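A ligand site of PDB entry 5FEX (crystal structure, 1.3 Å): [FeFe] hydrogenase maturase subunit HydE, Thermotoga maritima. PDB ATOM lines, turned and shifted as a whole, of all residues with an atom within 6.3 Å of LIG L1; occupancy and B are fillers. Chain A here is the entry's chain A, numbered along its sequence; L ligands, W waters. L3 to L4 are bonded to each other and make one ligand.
NH2 of Arg 190 is in salt-bridge range of O1 of LIG L1 (3.0 Å). The backbone carbonyl oxygen of Ser 118 sits close to a nitrogen (N1) of LIG L1 (3.3 Å). An iron atom (FE1) of LG2 L2 is bound by the side-chain sulfur (SG) of Cys 80. The side-chain sulfur (SG) of Cys 73 binds an iron atom (FE2) of LG2 L2 (2.2 Å). The backbone NH (N) of Cys 77 lies close to a sulfur (S4) of LG2 L2, 3.8 Å away. An iron atom (FE3) of LG2 L2 is bound by the side-chain sulfur (SG) of Cys 77 (2.4 Å). The side-chain carboxylate (OE2) of Glu 171 lies within hydrogen-bond range of an oxygen (O3) of LG3 L3. An oxygen (O2) of LG3 L3 sits at hydrogen-bond distance from the guanidinium group of Arg 169, 3.1 Å away. The backbone carbonyl oxygen of Tyr 79 sits at hydrogen-bond distance from a nitrogen (N5) of LG3 L3, 2.9 Å away.
Residues that only touch LIG L1: Tyr 313 (3.0 Å), Ser 146 (3.6 Å), Leu 315 (3.6 Å), Gly 148 (3.6 Å), Gln 117 (3.7 Å) and Leu 168 (3.8 Å). Hydrophobic or aromatic side chains that line LIG L1: Leu 168, Tyr 313 and Leu 315. The nearest printed residue that does not touch LIG L1 is Leu 147 (4.1 Å).
Water W4 lies within hydrogen-bond range of O of Leu 167, O1 of LIG L1, N of Gly 148, OG of Ser 146 and N of Leu 147. Water W1 lies within hydrogen-bond range of O3 of LG3 L3 (2.8 Å), O1 of LIG L1 (2.9 Å) and N of Arg 169 (3.0 Å). Water W2 lies within hydrogen-bond range of OE2 of Glu 120 (2.7 Å), NH1 of Arg 190 (2.8 Å), S1 of LG2 L2 (3.2 Å), NH2 of Arg 182 (3.3 Å) and O1 of LIG L1 (3.5 Å). Water W3 lies within hydrogen-bond range of OH of Tyr 79, OE2 of Glu 171, NE of Arg 182 and S2 of LG2 L2.
NH2 of Arg 190 lies within salt-bridge range of OE2 of Glu 171 (3.1 Å). O of Arg 169 lies within hydrogen-bond range of NE of Arg 190 (2.7 Å). The side-chain carboxylate (OE2) of Glu 149 lies within salt-bridge range of the guanidinium group (NH1) of Arg 190 (2.9 Å). OE1 of Gln 117 sits at hydrogen-bond distance from OH of Tyr 313 (3.0 Å). The backbone NH of Ser 118 lies within hydrogen-bond range of the backbone carbonyl oxygen of Ser 146 (3.3 Å). The side-chain hydroxyl (OG) of Ser 146 is in hydrogen-bond range of the side-chain amide nitrogen (NE2) of Gln 117 (3.1 Å). O of Leu 167 is in hydrogen-bond range of OG of Ser 146 (3.4 Å).
An oxygen (O2) of LIG L1 binds an iron atom (FE4) of LG2 L2 (2.2 Å).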
ATOM      1  N   CYS A  73     -35.184  24.143  -6.274  1.00  0.00           N
ATOM      2  CA  CYS A  73     -33.836  24.478  -6.722  1.00  0.00           C
ATOM      3  C   CYS A  73     -33.841  25.624  -7.738  1.00  0.00           C
ATOM      4  O   CYS A  73     -34.711  25.729  -8.632  1.00  0.00           O
ATOM      5  CB  CYS A  73     -33.162  23.252  -7.432  1.00  0.00           C
ATOM      6  SG  CYS A  73     -31.362  23.520  -7.560  1.00  0.00           S
ATOM      7  N   CYS A  77     -29.361  22.045 -13.716  1.00  0.00           N
ATOM      8  CA  CYS A  77     -28.495  20.973 -14.200  1.00  0.00           C
ATOM      9  C   CYS A  77     -29.222  20.011 -15.107  1.00  0.00           C
ATOM     10  O   CYS A  77     -30.348  19.606 -14.836  1.00  0.00           O
ATOM     11  CB  CYS A  77     -27.849  20.225 -12.948  1.00  0.00           C
ATOM     12  SG  CYS A  77     -27.091  21.271 -11.743  1.00  0.00           S
ATOM     13  N   TYR A  79     -29.015  16.948 -15.963  1.00  0.00           N
ATOM     14  CA  TYR A  79     -29.272  15.523 -15.548  1.00  0.00           C
ATOM     15  C   TYR A  79     -30.343  15.377 -14.477  1.00  0.00           C
ATOM     16  O   TYR A  79     -30.831  14.290 -14.211  1.00  0.00           O
ATOM     17  CB  TYR A  79     -27.988  14.901 -15.049  1.00  0.00           C
ATOM     18  CG  TYR A  79     -27.162  15.732 -14.130  1.00  0.00           C
ATOM     19  CD1 TYR A  79     -27.449  15.831 -12.790  1.00  0.00           C
ATOM     20  CD2 TYR A  79     -26.061  16.452 -14.577  1.00  0.00           C
ATOM     21  CE1 TYR A  79     -26.690  16.632 -11.964  1.00  0.00           C
ATOM     22  CE2 TYR A  79     -25.279  17.256 -13.772  1.00  0.00           C
ATOM     23  CZ  TYR A  79     -25.608  17.359 -12.440  1.00  0.00           C
ATOM     24  OH  TYR A  79     -24.843  18.184 -11.649  1.00  0.00           O
ATOM     25  N   CYS A  80     -30.674  16.487 -13.770  1.00  0.00           N
ATOM     26  CA  CYS A  80     -31.353  16.356 -12.465  1.00  0.00           C
ATOM     27  C   CYS A  80     -32.857  16.610 -12.510  1.00  0.00           C
ATOM     28  O   CYS A  80     -33.322  17.655 -13.037  1.00  0.00           O
ATOM     29  CB  CYS A  80     -30.790  17.388 -11.514  1.00  0.00           C
ATOM     30  SG  CYS A  80     -31.444  17.289  -9.809  1.00  0.00           S
ATOM     31  N   LEU A  82     -34.745  17.656 -10.264  1.00  0.00           N
ATOM     32  CA  LEU A  82     -35.104  18.826  -9.523  1.00  0.00           C
ATOM     33  C   LEU A  82     -34.783  20.133 -10.227  1.00  0.00           C
ATOM     34  O   LEU A  82     -35.094  21.207  -9.681  1.00  0.00           O
ATOM     35  CB  LEU A  82     -34.432  18.881  -8.118  1.00  0.00           C
ATOM     36  CG  LEU A  82     -34.675  17.642  -7.194  1.00  0.00           C
ATOM     37  CD1 LEU A  82     -34.170  17.991  -5.780  1.00  0.00           C
ATOM     38  CD2 LEU A  82     -36.073  17.008  -7.227  1.00  0.00           C
ATOM     39  N   GLN A 117     -30.004  17.465   3.166  1.00  0.00           N
ATOM     40  CA  GLN A 117     -29.799  17.658   1.751  1.00  0.00           C
ATOM     41  C   GLN A 117     -30.987  18.406   1.148  1.00  0.00           C
ATOM     42  O   GLN A 117     -32.136  18.167   1.562  1.00  0.00           O
ATOM     43  CB  GLN A 117     -29.554  16.353   0.992  1.00  0.00           C
ATOM     44  CG  GLN A 117     -29.096  16.592  -0.467  1.00  0.00           C
ATOM     45  CD  GLN A 117     -28.791  15.353  -1.203  1.00  0.00           C
ATOM     46  OE1 GLN A 117     -29.757  14.738  -1.768  1.00  0.00           O
ATOM     47  NE2 GLN A 117     -27.579  14.954  -1.315  1.00  0.00           N
ATOM     48  N   SER A 118     -30.753  19.226   0.161  1.00  0.00           N
ATOM     49  CA  SER A 118     -31.809  19.892  -0.548  1.00  0.00           C
ATOM     50  C   SER A 118     -31.352  20.273  -1.928  1.00  0.00           C
ATOM     51  O   SER A 118     -30.168  20.266  -2.270  1.00  0.00           O
ATOM     52  CB  SER A 118     -32.302  21.136   0.186  1.00  0.00           C
ATOM     53  OG  SER A 118     -31.223  22.099   0.354  1.00  0.00           O
ATOM     54  N   GLY A 119     -32.367  20.698  -2.759  1.00  0.00           N
ATOM     55  CA  GLY A 119     -32.042  21.567  -3.890  1.00  0.00           C
ATOM     56  C   GLY A 119     -31.413  22.846  -3.385  1.00  0.00           C
ATOM     57  O   GLY A 119     -31.409  23.149  -2.182  1.00  0.00           O
ATOM     58  N   GLU A 120     -30.831  23.599  -4.311  1.00  0.00           N
ATOM     59  CA  GLU A 120     -30.356  24.942  -3.935  1.00  0.00           C
ATOM     60  C   GLU A 120     -31.515  25.899  -3.757  1.00  0.00           C
ATOM     61  O   GLU A 120     -31.922  26.658  -4.681  1.00  0.00           O
ATOM     62  CB  GLU A 120     -29.341  25.504  -4.953  1.00  0.00           C
ATOM     63  CG  GLU A 120     -28.028  24.780  -4.978  1.00  0.00           C
ATOM     64  CD  GLU A 120     -26.936  25.496  -5.716  1.00  0.00           C
ATOM     65  OE1 GLU A 120     -27.159  26.660  -6.147  1.00  0.00           O
ATOM     66  OE2 GLU A 120     -25.817  24.932  -5.893  1.00  0.00           O
ATOM     67  N   SER A 146     -25.524  19.081   2.656  1.00  0.00           N
ATOM     68  CA  SER A 146     -25.372  18.799   1.211  1.00  0.00           C
ATOM     69  C   SER A 146     -26.373  19.741   0.517  1.00  0.00           C
ATOM     70  O   SER A 146     -27.445  19.370   0.113  1.00  0.00           O
ATOM     71  CB  SER A 146     -25.627  17.344   0.898  1.00  0.00           C
ATOM     72  OG  SER A 146     -25.445  17.062  -0.474  1.00  0.00           O
ATOM     73  N   LEU A 147     -26.001  21.034   0.433  1.00  0.00           N
ATOM     74  CA  LEU A 147     -26.907  22.115   0.041  1.00  0.00           C
ATOM     75  C   LEU A 147     -26.466  22.811  -1.247  1.00  0.00           C
ATOM     76  O   LEU A 147     -27.135  23.735  -1.703  1.00  0.00           O
ATOM     77  CB  LEU A 147     -27.035  23.178   1.161  1.00  0.00           C
ATOM     78  CG  LEU A 147     -27.310  22.620   2.535  1.00  0.00           C
ATOM     79  CD1 LEU A 147     -27.350  23.748   3.537  1.00  0.00           C
ATOM     80  CD2 LEU A 147     -28.558  21.763   2.596  1.00  0.00           C
ATOM     81  N   GLY A 148     -25.382  22.354  -1.887  1.00  0.00           N
ATOM     82  CA  GLY A 148     -24.906  22.982  -3.123  1.00  0.00           C
ATOM     83  C   GLY A 148     -23.887  24.083  -2.875  1.00  0.00           C
ATOM     84  O   GLY A 148     -23.195  24.141  -1.895  1.00  0.00           O
ATOM     85  N   GLU A 149     -23.827  24.937  -3.946  1.00  0.00           N
ATOM     86  CA  GLU A 149     -22.844  26.048  -3.981  1.00  0.00           C
ATOM     87  C   GLU A 149     -23.429  27.366  -3.413  1.00  0.00           C
ATOM     88  O   GLU A 149     -24.473  27.810  -3.862  1.00  0.00           O
ATOM     89  CB  GLU A 149     -22.550  26.332  -5.455  1.00  0.00           C
ATOM     90  CG  GLU A 149     -21.851  25.149  -6.154  1.00  0.00           C
ATOM     91  CD  GLU A 149     -21.713  25.251  -7.664  1.00  0.00           C
ATOM     92  OE1 GLU A 149     -21.456  26.381  -8.144  1.00  0.00           O
ATOM     93  OE2 GLU A 149     -21.903  24.214  -8.343  1.00  0.00           O
ATOM     94  N   LEU A 167     -21.017  17.596   1.876  1.00  0.00           N
ATOM     95  CA  LEU A 167     -20.956  16.795   0.663  1.00  0.00           C
ATOM     96  C   LEU A 167     -21.194  17.717  -0.549  1.00  0.00           C
ATOM     97  O   LEU A 167     -22.291  18.316  -0.624  1.00  0.00           O
ATOM     98  CB  LEU A 167     -22.019  15.715   0.648  1.00  0.00           C
ATOM     99  CG  LEU A 167     -22.087  14.852   1.864  1.00  0.00           C
ATOM    100  CD1 LEU A 167     -23.262  13.856   1.720  1.00  0.00           C
ATOM    101  CD2 LEU A 167     -20.726  14.164   2.133  1.00  0.00           C
ATOM    102  N   LEU A 168     -20.257  17.788  -1.483  1.00  0.00           N
ATOM    103  CA  LEU A 168     -20.382  18.579  -2.700  1.00  0.00           C
ATOM    104  C   LEU A 168     -19.697  17.819  -3.834  1.00  0.00           C
ATOM    105  O   LEU A 168     -18.516  18.035  -4.127  1.00  0.00           O
ATOM    106  CB  LEU A 168     -19.832  19.988  -2.508  1.00  0.00           C
ATOM    107  CG  LEU A 168     -20.194  20.965  -3.619  1.00  0.00           C
ATOM    108  CD1 LEU A 168     -21.648  21.387  -3.566  1.00  0.00           C
ATOM    109  CD2 LEU A 168     -19.311  22.253  -3.449  1.00  0.00           C
ATOM    110  N   ARG A 169     -20.441  16.900  -4.426  1.00  0.00           N
ATOM    111  CA  ARG A 169     -19.834  16.090  -5.497  1.00  0.00           C
ATOM    112  C   ARG A 169     -19.243  17.029  -6.547  1.00  0.00           C
ATOM    113  O   ARG A 169     -19.912  18.009  -6.945  1.00  0.00           O
ATOM    114  CB  ARG A 169     -20.844  15.156  -6.110  1.00  0.00           C
ATOM    115  CG  ARG A 169     -21.228  14.028  -5.198  1.00  0.00           C
ATOM    116  CD  ARG A 169     -22.006  13.062  -6.091  1.00  0.00           C
ATOM    117  NE  ARG A 169     -22.553  12.018  -5.310  1.00  0.00           N
ATOM    118  CZ  ARG A 169     -23.132  10.937  -5.865  1.00  0.00           C
ATOM    119  NH1 ARG A 169     -23.338  10.881  -7.171  1.00  0.00           N
ATOM    120  NH2 ARG A 169     -23.460   9.949  -5.073  1.00  0.00           N
ATOM    121  N   GLU A 171     -18.926  16.138  -9.627  1.00  0.00           N
ATOM    122  CA  GLU A 171     -19.795  15.720 -10.724  1.00  0.00           C
ATOM    123  C   GLU A 171     -19.013  15.182 -11.952  1.00  0.00           C
ATOM    124  O   GLU A 171     -19.265  14.066 -12.374  1.00  0.00           O
ATOM    125  CB  GLU A 171     -20.803  16.836 -11.137  1.00  0.00           C
ATOM    126  CG  GLU A 171     -21.599  17.470  -9.989  1.00  0.00           C
ATOM    127  CD  GLU A 171     -22.468  16.535  -9.217  1.00  0.00           C
ATOM    128  OE1 GLU A 171     -22.465  15.293  -9.465  1.00  0.00           O
ATOM    129  OE2 GLU A 171     -23.188  17.069  -8.282  1.00  0.00           O
ATOM    130  N   ARG A 182     -24.038  21.810 -16.408  1.00  0.00           N
ATOM    131  CA  ARG A 182     -24.346  22.616 -15.211  1.00  0.00           C
ATOM    132  C   ARG A 182     -24.208  24.118 -15.627  1.00  0.00           C
ATOM    133  O   ARG A 182     -23.272  24.795 -15.298  1.00  0.00           O
ATOM    134  CB  ARG A 182     -23.461  22.248 -14.036  1.00  0.00           C
ATOM    135  CG  ARG A 182     -23.446  20.749 -13.778  1.00  0.00           C
ATOM    136  CD  ARG A 182     -22.723  20.339 -12.491  1.00  0.00           C
ATOM    137  NE  ARG A 182     -23.518  20.833 -11.355  1.00  0.00           N
ATOM    138  CZ  ARG A 182     -23.164  21.819 -10.519  1.00  0.00           C
ATOM    139  NH1 ARG A 182     -21.984  22.341 -10.514  1.00  0.00           N
ATOM    140  NH2 ARG A 182     -24.116  22.243  -9.679  1.00  0.00           N
ATOM    141  N   ARG A 190     -17.064  25.069  -8.619  1.00  0.00           N
ATOM    142  CA  ARG A 190     -17.265  23.859  -7.810  1.00  0.00           C
ATOM    143  C   ARG A 190     -16.060  23.526  -6.968  1.00  0.00           C
ATOM    144  O   ARG A 190     -16.117  23.264  -5.768  1.00  0.00           O
ATOM    145  CB  ARG A 190     -17.662  22.705  -8.733  1.00  0.00           C
ATOM    146  CG  ARG A 190     -18.306  21.503  -8.020  1.00  0.00           C
ATOM    147  CD  ARG A 190     -19.755  21.818  -7.659  1.00  0.00           C
ATOM    148  NE  ARG A 190     -20.508  20.631  -7.286  1.00  0.00           N
ATOM    149  CZ  ARG A 190     -21.781  20.657  -6.874  1.00  0.00           C
ATOM    150  NH1 ARG A 190     -22.476  21.789  -6.913  1.00  0.00           N
ATOM    151  NH2 ARG A 190     -22.372  19.532  -6.497  1.00  0.00           N
ATOM    152  N   TYR A 313     -38.873  13.782  -4.055  1.00  0.00           N
ATOM    153  CA  TYR A 313     -37.468  14.070  -4.191  1.00  0.00           C
ATOM    154  C   TYR A 313     -36.819  13.018  -5.089  1.00  0.00           C
ATOM    155  O   TYR A 313     -36.225  12.053  -4.580  1.00  0.00           O
ATOM    156  CB  TYR A 313     -36.805  14.149  -2.805  1.00  0.00           C
ATOM    157  CG  TYR A 313     -35.469  14.860  -2.799  1.00  0.00           C
ATOM    158  CD1 TYR A 313     -35.389  16.226  -2.449  1.00  0.00           C
ATOM    159  CD2 TYR A 313     -34.296  14.195  -3.061  1.00  0.00           C
ATOM    160  CE1 TYR A 313     -34.198  16.877  -2.398  1.00  0.00           C
ATOM    161  CE2 TYR A 313     -33.076  14.815  -2.962  1.00  0.00           C
ATOM    162  CZ  TYR A 313     -33.028  16.171  -2.609  1.00  0.00           C
ATOM    163  OH  TYR A 313     -31.825  16.839  -2.441  1.00  0.00           O
ATOM    164  N   LEU A 315     -34.245  12.754  -7.918  1.00  0.00           N
ATOM    165  CA  LEU A 315     -33.201  13.253  -8.765  1.00  0.00           C
ATOM    166  C   LEU A 315     -33.177  12.446 -10.005  1.00  0.00           C
ATOM    167  O   LEU A 315     -32.877  12.977 -11.064  1.00  0.00           O
ATOM    168  CB  LEU A 315     -31.841  13.131  -8.034  1.00  0.00           C
ATOM    169  CG  LEU A 315     -31.694  13.709  -6.605  1.00  0.00           C
ATOM    170  CD1 LEU A 315     -30.295  13.611  -6.188  1.00  0.00           C
ATOM    171  CD2 LEU A 315     -32.211  15.028  -6.525  1.00  0.00           C
HETATM  172  N1  LIG L   1     -28.149  20.460  -4.876  1.00  0.00           N
HETATM  173  C1  LIG L   1     -26.969  19.935  -4.089  1.00  0.00           C
HETATM  174  C2  LIG L   1     -25.876  19.643  -5.077  1.00  0.00           C
HETATM  175  O1  LIG L   1     -24.710  19.457  -4.678  1.00  0.00           O
HETATM  176  C3  LIG L   1     -27.376  18.662  -3.381  1.00  0.00           C
HETATM  177  C4  LIG L   1     -27.322  17.326  -4.192  1.00  0.00           C
HETATM  178  S1  LIG L   1     -28.444  17.277  -5.581  1.00  0.00           S
HETATM  179  C5  LIG L   1     -29.987  17.231  -4.736  1.00  0.00           C
HETATM  180  O2  LIG L   1     -26.211  19.593  -6.347  1.00  0.00           O
HETATM  181 FE1  LG2 L   2     -30.282  19.063  -8.969  1.00  0.00          FE
HETATM  182 FE2  LG2 L   2     -30.326  21.644  -8.200  1.00  0.00          FE
HETATM  183 FE3  LG2 L   2     -28.307  20.723  -9.802  1.00  0.00          FE
HETATM  184 FE4  LG2 L   2     -28.348  19.778  -7.011  1.00  0.00          FE
HETATM  185  S1  LG2 L   2     -28.033  22.034  -7.952  1.00  0.00           S
HETATM  186  S2  LG2 L   2     -28.040  18.556  -9.004  1.00  0.00           S
HETATM  187  S3  LG2 L   2     -30.740  19.798  -6.908  1.00  0.00           S
HETATM  188  S4  LG2 L   2     -30.549  20.925 -10.338  1.00  0.00           S
HETATM  189  N1  LG3 L   3     -28.627  10.258 -11.919  1.00  0.00           N
HETATM  190  C1  LG3 L   3     -27.854   9.911 -10.899  1.00  0.00           C
HETATM  191  N2  LG3 L   3     -27.352  10.701  -9.992  1.00  0.00           N
HETATM  192  C2  LG3 L   3     -27.824  11.937  -9.957  1.00  0.00           C
HETATM  193  N3  LG3 L   3     -27.541  12.992  -9.192  1.00  0.00           N
HETATM  194  C3  LG3 L   3     -28.292  14.054  -9.628  1.00  0.00           C
HETATM  195  N4  LG3 L   3     -29.074  13.725 -10.702  1.00  0.00           N
HETATM  196  C4  LG3 L   3     -28.762  12.408 -10.940  1.00  0.00           C
HETATM  197  C5  LG3 L   3     -29.199  11.472 -11.923  1.00  0.00           C
HETATM  198  N5  LG3 L   3     -30.068  11.846 -12.917  1.00  0.00           N
HETATM  199  C6  LG3 L   3     -26.440  12.964  -8.229  1.00  0.00           C
HETATM  200  C7  LG3 L   3     -25.454  14.149  -8.437  1.00  0.00           C
HETATM  201  C8  LG3 L   3     -25.618  14.915  -7.129  1.00  0.00           C
HETATM  202  C9  LG3 L   3     -25.846  13.711  -6.132  1.00  0.00           C
HETATM  203  C10 LG3 L   3     -26.482  13.986  -4.800  1.00  0.00           C
HETATM  204  O1  LG3 L   3     -26.882  12.968  -6.906  1.00  0.00           O
HETATM  205  O2  LG3 L   3     -24.153  13.526  -8.535  1.00  0.00           O
HETATM  206  O3  LG3 L   3     -24.416  15.544  -6.657  1.00  0.00           O
HETATM  207  N1  LG4 L   4     -26.202   9.268  -2.903  1.00  0.00           N
HETATM  208  C1  LG4 L   4     -27.439   9.819  -3.497  1.00  0.00           C
HETATM  209  C2  LG4 L   4     -27.206  10.985  -4.409  1.00  0.00           C
HETATM  210 SE1  LG4 L   4     -26.200  12.421  -3.467  1.00  0.00          SE
HETATM  211  C3  LG4 L   4     -28.043   8.761  -4.308  1.00  0.00           C
HETATM  212  O1  LG4 L   4     -27.380   7.873  -4.921  1.00  0.00           O
HETATM  213  O2  LG4 L   4     -29.291   8.817  -4.373  1.00  0.00           O
HETATM  214  O   HOH W   1     -23.464  16.903  -4.421  1.00  0.00           O
HETATM  215  O   HOH W   2     -25.158  22.391  -6.513  1.00  0.00           O
HETATM  216  O   HOH W   3     -24.851  19.075  -9.111  1.00  0.00           O
HETATM  217  O   HOH W   4     -24.298  19.598  -1.942  1.00  0.00           O
